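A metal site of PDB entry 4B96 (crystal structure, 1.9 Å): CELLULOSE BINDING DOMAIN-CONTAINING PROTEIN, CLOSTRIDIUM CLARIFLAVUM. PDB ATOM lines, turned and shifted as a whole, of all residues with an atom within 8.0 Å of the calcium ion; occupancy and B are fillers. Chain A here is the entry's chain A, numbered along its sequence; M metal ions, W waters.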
ATOM      1  N   LEU A  16      22.906  23.712  18.189  1.00  0.00           N
ATOM      2  CA  LEU A  16      21.611  23.809  17.500  1.00  0.00           C
ATOM      3  C   LEU A  16      21.587  25.099  16.639  1.00  0.00           C
ATOM      4  O   LEU A  16      21.109  25.103  15.528  1.00  0.00           O
ATOM      5  CB  LEU A  16      20.470  23.839  18.529  1.00  0.00           C
ATOM      6  CG  LEU A  16      20.260  22.537  19.316  1.00  0.00           C
ATOM      7  CD1 LEU A  16      18.908  22.581  19.970  1.00  0.00           C
ATOM      8  CD2 LEU A  16      20.386  21.333  18.323  1.00  0.00           C
ATOM      9  N   ILE A  21      26.088  25.356   8.210  1.00  0.00           N
ATOM     10  CA  ILE A  21      25.723  23.979   8.278  1.00  0.00           C
ATOM     11  C   ILE A  21      26.832  23.200   7.556  1.00  0.00           C
ATOM     12  O   ILE A  21      27.208  23.574   6.436  1.00  0.00           O
ATOM     13  CB  ILE A  21      24.356  23.736   7.597  1.00  0.00           C
ATOM     14  CG1 ILE A  21      23.238  24.251   8.548  1.00  0.00           C
ATOM     15  CG2 ILE A  21      24.160  22.192   7.315  1.00  0.00           C
ATOM     16  CD1 ILE A  21      21.815  24.224   7.857  1.00  0.00           C
ATOM     17  N   TYR A  45      19.330  17.298   3.730  1.00  0.00           N
ATOM     18  CA  TYR A  45      17.988  17.862   3.943  1.00  0.00           C
ATOM     19  C   TYR A  45      17.970  18.766   5.132  1.00  0.00           C
ATOM     20  O   TYR A  45      18.442  18.392   6.224  1.00  0.00           O
ATOM     21  CB  TYR A  45      16.999  16.747   4.213  1.00  0.00           C
ATOM     22  CG  TYR A  45      16.911  15.850   3.024  1.00  0.00           C
ATOM     23  CD1 TYR A  45      15.982  16.118   2.019  1.00  0.00           C
ATOM     24  CD2 TYR A  45      17.730  14.728   2.916  1.00  0.00           C
ATOM     25  CE1 TYR A  45      15.906  15.347   0.920  1.00  0.00           C
ATOM     26  CE2 TYR A  45      17.627  13.878   1.797  1.00  0.00           C
ATOM     27  CZ  TYR A  45      16.738  14.202   0.819  1.00  0.00           C
ATOM     28  OH  TYR A  45      16.622  13.427  -0.301  1.00  0.00           O
ATOM     29  N   PHE A  46      17.379  19.956   4.954  1.00  0.00           N
ATOM     30  CA  PHE A  46      17.278  20.904   6.053  1.00  0.00           C
ATOM     31  C   PHE A  46      16.011  21.741   5.939  1.00  0.00           C
ATOM     32  O   PHE A  46      15.344  21.795   4.875  1.00  0.00           O
ATOM     33  CB  PHE A  46      18.535  21.757   6.141  1.00  0.00           C
ATOM     34  CG  PHE A  46      18.726  22.692   4.975  1.00  0.00           C
ATOM     35  CD1 PHE A  46      19.253  22.232   3.748  1.00  0.00           C
ATOM     36  CD2 PHE A  46      18.410  24.062   5.103  1.00  0.00           C
ATOM     37  CE1 PHE A  46      19.458  23.096   2.654  1.00  0.00           C
ATOM     38  CE2 PHE A  46      18.615  24.940   4.000  1.00  0.00           C
ATOM     39  CZ  PHE A  46      19.100  24.465   2.779  1.00  0.00           C
ATOM     40  N   LYS A  47      15.630  22.336   7.059  1.00  0.00           N
ATOM     41  CA  LYS A  47      14.422  23.177   7.076  1.00  0.00           C
ATOM     42  C   LYS A  47      14.895  24.606   7.347  1.00  0.00           C
ATOM     43  O   LYS A  47      15.466  24.869   8.391  1.00  0.00           O
ATOM     44  CB  LYS A  47      13.505  22.717   8.199  1.00  0.00           C
ATOM     45  CG  LYS A  47      12.146  23.460   8.230  1.00  0.00           C
ATOM     46  CD  LYS A  47      11.257  22.839   9.352  1.00  0.00           C
ATOM     47  CE  LYS A  47       9.810  23.393   9.336  1.00  0.00           C
ATOM     48  NZ  LYS A  47       9.798  24.830   9.623  1.00  0.00           N
ATOM     49  N   ASP A  48      14.633  25.539   6.440  1.00  0.00           N
ATOM     50  CA  ASP A  48      15.074  26.915   6.679  1.00  0.00           C
ATOM     51  C   ASP A  48      14.366  27.814   5.683  1.00  0.00           C
ATOM     52  O   ASP A  48      14.057  27.394   4.571  1.00  0.00           O
ATOM     53  CB  ASP A  48      16.584  27.001   6.500  1.00  0.00           C
ATOM     54  CG  ASP A  48      17.120  28.331   6.997  1.00  0.00           C
ATOM     55  OD1 ASP A  48      17.209  28.497   8.237  1.00  0.00           O
ATOM     56  OD2 ASP A  48      17.450  29.184   6.134  1.00  0.00           O
ATOM     57  N   ASP A  49      14.080  29.026   6.073  1.00  0.00           N
ATOM     58  CA  ASP A  49      13.250  29.901   5.231  1.00  0.00           C
ATOM     59  C   ASP A  49      14.014  31.108   4.654  1.00  0.00           C
ATOM     60  O   ASP A  49      13.393  32.046   4.134  1.00  0.00           O
ATOM     61  CB  ASP A  49      12.033  30.333   6.031  1.00  0.00           C
ATOM     62  CG  ASP A  49      10.703  29.823   5.400  1.00  0.00           C
ATOM     63  OD1 ASP A  49      10.675  29.446   4.181  1.00  0.00           O
ATOM     64  OD2 ASP A  49       9.679  29.876   6.114  1.00  0.00           O
ATOM     65  N   SER A  82       9.875  26.115   3.517  1.00  0.00           N
ATOM     66  CA  SER A  82      10.999  25.884   4.419  1.00  0.00           C
ATOM     67  C   SER A  82      11.688  24.522   4.254  1.00  0.00           C
ATOM     68  O   SER A  82      12.844  24.372   4.633  1.00  0.00           O
ATOM     69  CB  SER A  82      10.501  26.084   5.842  1.00  0.00           C
ATOM     70  OG  SER A  82       9.631  25.055   6.205  1.00  0.00           O
ATOM     71  N   ARG A 109      23.846  31.334   5.268  1.00  0.00           N
ATOM     72  CA  ARG A 109      22.919  32.335   4.750  1.00  0.00           C
ATOM     73  C   ARG A 109      23.760  33.501   4.255  1.00  0.00           C
ATOM     74  O   ARG A 109      24.746  33.910   4.918  1.00  0.00           O
ATOM     75  CB  ARG A 109      21.971  32.854   5.842  1.00  0.00           C
ATOM     76  CG  ARG A 109      21.060  31.768   6.400  1.00  0.00           C
ATOM     77  CD  ARG A 109      20.210  32.438   7.448  1.00  0.00           C
ATOM     78  NE  ARG A 109      19.115  31.565   7.859  1.00  0.00           N
ATOM     79  CZ  ARG A 109      18.125  31.983   8.661  1.00  0.00           C
ATOM     80  NH1 ARG A 109      18.155  33.224   9.172  1.00  0.00           N
ATOM     81  NH2 ARG A 109      17.111  31.161   8.978  1.00  0.00           N
ATOM     82  N   GLU A 114      22.006  33.099  11.717  1.00  0.00           N
ATOM     83  CA  GLU A 114      22.153  31.697  12.140  1.00  0.00           C
ATOM     84  C   GLU A 114      21.026  30.787  11.667  1.00  0.00           C
ATOM     85  O   GLU A 114      19.841  31.188  11.655  1.00  0.00           O
ATOM     86  CB  GLU A 114      22.197  31.615  13.673  1.00  0.00           C
ATOM     87  CG  GLU A 114      23.559  32.032  14.270  1.00  0.00           C
ATOM     88  CD  GLU A 114      23.574  31.954  15.818  1.00  0.00           C
ATOM     89  OE1 GLU A 114      22.507  32.131  16.462  1.00  0.00           O
ATOM     90  OE2 GLU A 114      24.662  31.710  16.373  1.00  0.00           O
ATOM     91  N   PHE A 115      21.393  29.564  11.311  1.00  0.00           N
ATOM     92  CA  PHE A 115      20.419  28.490  11.155  1.00  0.00           C
ATOM     93  C   PHE A 115      20.015  27.935  12.537  1.00  0.00           C
ATOM     94  O   PHE A 115      20.778  28.050  13.510  1.00  0.00           O
ATOM     95  CB  PHE A 115      21.032  27.305  10.404  1.00  0.00           C
ATOM     96  CG  PHE A 115      21.435  27.625   9.019  1.00  0.00           C
ATOM     97  CD1 PHE A 115      20.492  27.733   8.010  1.00  0.00           C
ATOM     98  CD2 PHE A 115      22.797  27.733   8.688  1.00  0.00           C
ATOM     99  CE1 PHE A 115      20.877  27.994   6.661  1.00  0.00           C
ATOM    100  CE2 PHE A 115      23.201  28.005   7.368  1.00  0.00           C
ATOM    101  CZ  PHE A 115      22.246  28.133   6.335  1.00  0.00           C
ATOM    102  N   ASN A 116      18.836  27.286  12.593  1.00  0.00           N
ATOM    103  CA  ASN A 116      18.459  26.430  13.703  1.00  0.00           C
ATOM    104  C   ASN A 116      18.463  25.017  13.142  1.00  0.00           C
ATOM    105  O   ASN A 116      17.593  24.667  12.316  1.00  0.00           O
ATOM    106  CB  ASN A 116      17.047  26.809  14.187  1.00  0.00           C
ATOM    107  CG  ASN A 116      16.486  25.793  15.221  1.00  0.00           C
ATOM    108  OD1 ASN A 116      17.212  24.952  15.753  1.00  0.00           O
ATOM    109  ND2 ASN A 116      15.182  25.860  15.468  1.00  0.00           N
ATOM    110  N   GLN A 117      19.432  24.210  13.528  1.00  0.00           N
ATOM    111  CA  GLN A 117      19.624  22.926  12.931  1.00  0.00           C
ATOM    112  C   GLN A 117      18.715  21.864  13.537  1.00  0.00           C
ATOM    113  O   GLN A 117      18.665  20.729  13.028  1.00  0.00           O
ATOM    114  CB  GLN A 117      21.050  22.481  13.157  1.00  0.00           C
ATOM    115  CG  GLN A 117      22.082  23.452  12.603  1.00  0.00           C
ATOM    116  CD  GLN A 117      23.478  22.796  12.489  1.00  0.00           C
ATOM    117  OE1 GLN A 117      23.721  22.098  11.536  1.00  0.00           O
ATOM    118  NE2 GLN A 117      24.339  23.020  13.470  1.00  0.00           N
ATOM    119  N   GLU A 118      18.033  22.231  14.603  1.00  0.00           N
ATOM    120  CA  GLU A 118      17.292  21.214  15.381  1.00  0.00           C
ATOM    121  C   GLU A 118      16.233  20.466  14.590  1.00  0.00           C
ATOM    122  O   GLU A 118      15.944  19.311  14.892  1.00  0.00           O
ATOM    123  CB  GLU A 118      16.663  21.824  16.628  1.00  0.00           C
ATOM    124  CG  GLU A 118      16.172  20.729  17.599  1.00  0.00           C
ATOM    125  CD  GLU A 118      15.608  21.285  18.907  1.00  0.00           C
ATOM    126  OE1 GLU A 118      15.043  22.421  18.893  1.00  0.00           O
ATOM    127  OE2 GLU A 118      15.737  20.566  19.939  1.00  0.00           O
ATOM    128  N   ASP A 119      15.653  21.115  13.583  1.00  0.00           N
ATOM    129  CA  ASP A 119      14.577  20.516  12.819  1.00  0.00           C
ATOM    130  C   ASP A 119      15.058  20.089  11.425  1.00  0.00           C
ATOM    131  O   ASP A 119      14.232  19.882  10.515  1.00  0.00           O
ATOM    132  CB  ASP A 119      13.429  21.539  12.739  1.00  0.00           C
ATOM    133  CG  ASP A 119      13.906  22.938  12.195  1.00  0.00           C
ATOM    134  OD1 ASP A 119      15.073  23.086  11.691  1.00  0.00           O
ATOM    135  OD2 ASP A 119      13.069  23.888  12.270  1.00  0.00           O
ATOM    136  N   ASP A 120      16.376  19.950  11.250  1.00  0.00           N
ATOM    137  CA  ASP A 120      16.906  19.590   9.934  1.00  0.00           C
ATOM    138  C   ASP A 120      17.054  18.070   9.843  1.00  0.00           C
ATOM    139  O   ASP A 120      17.742  17.426  10.687  1.00  0.00           O
ATOM    140  CB  ASP A 120      18.301  20.227   9.712  1.00  0.00           C
ATOM    141  CG  ASP A 120      18.261  21.728   9.646  1.00  0.00           C
ATOM    142  OD1 ASP A 120      17.172  22.337   9.528  1.00  0.00           O
ATOM    143  OD2 ASP A 120      19.361  22.340   9.675  1.00  0.00           O
ATOM    144  N   TRP A 121      16.406  17.470   8.854  1.00  0.00           N
ATOM    145  CA  TRP A 121      16.420  16.005   8.748  1.00  0.00           C
ATOM    146  C   TRP A 121      17.874  15.439   8.767  1.00  0.00           C
ATOM    147  O   TRP A 121      18.148  14.427   9.413  1.00  0.00           O
ATOM    148  CB  TRP A 121      15.713  15.586   7.435  1.00  0.00           C
ATOM    149  CG  TRP A 121      15.596  14.054   7.159  1.00  0.00           C
ATOM    150  CD1 TRP A 121      16.402  13.292   6.337  1.00  0.00           C
ATOM    151  CD2 TRP A 121      14.628  13.161   7.712  1.00  0.00           C
ATOM    152  NE1 TRP A 121      15.985  11.965   6.357  1.00  0.00           N
ATOM    153  CE2 TRP A 121      14.879  11.868   7.171  1.00  0.00           C
ATOM    154  CE3 TRP A 121      13.546  13.331   8.589  1.00  0.00           C
ATOM    155  CZ2 TRP A 121      14.080  10.764   7.457  1.00  0.00           C
ATOM    156  CZ3 TRP A 121      12.754  12.239   8.873  1.00  0.00           C
ATOM    157  CH2 TRP A 121      13.034  10.960   8.326  1.00  0.00           C
ATOM    158  N   PHE A 123      20.628  16.522  10.095  1.00  0.00           N
ATOM    159  CA  PHE A 123      21.478  17.000  11.193  1.00  0.00           C
ATOM    160  C   PHE A 123      21.940  15.841  12.090  1.00  0.00           C
ATOM    161  O   PHE A 123      21.113  15.071  12.592  1.00  0.00           O
ATOM    162  CB  PHE A 123      20.730  18.012  12.014  1.00  0.00           C
ATOM    163  CG  PHE A 123      21.506  18.569  13.205  1.00  0.00           C
ATOM    164  CD1 PHE A 123      22.810  19.113  13.044  1.00  0.00           C
ATOM    165  CD2 PHE A 123      20.934  18.604  14.440  1.00  0.00           C
ATOM    166  CE1 PHE A 123      23.473  19.651  14.162  1.00  0.00           C
ATOM    167  CE2 PHE A 123      21.586  19.153  15.531  1.00  0.00           C
ATOM    168  CZ  PHE A 123      22.853  19.647  15.384  1.00  0.00           C
HETATM  169 CA    CA M   1      16.511  24.566  10.358  1.00  0.00          CA
HETATM  170  O   HOH W   1      17.060  26.984  10.316  1.00  0.00           O
HETATM  171  O   HOH W   2      18.561  24.783   9.199  1.00  0.00           O
HETATM  172  O   HOH W   3      14.345  25.813  11.077  1.00  0.00           O
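The side-chain amino group of Lys 47 lies within hydrogen-bond range of the side-chain hydroxyl of Ser 82 (3.4 Å). The side-chain amide oxygen of Asn 116 is in hydrogen-bond range of the backbone NH of Glu 118.
Four residues have an atom within 4 Å of the calcium ion: Lys 47, Asn 116, Asp 119 and Asp 120. The nearest printed residue that does not touch the calcium ion is Gln 117 (4.3 Å).
The calcium ion is bound by O of Asn 116, O of Lys 47, water W2, OD1 of Asp 119, OD1 of Asp 120, water W1 and water W3. The calcium ion has seven donor atoms within binding distance.
Water W1 lies within hydrogen-bond range of OD1 of Asp 48 (2.6 Å) and N of Asn 116 (2.9 Å).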
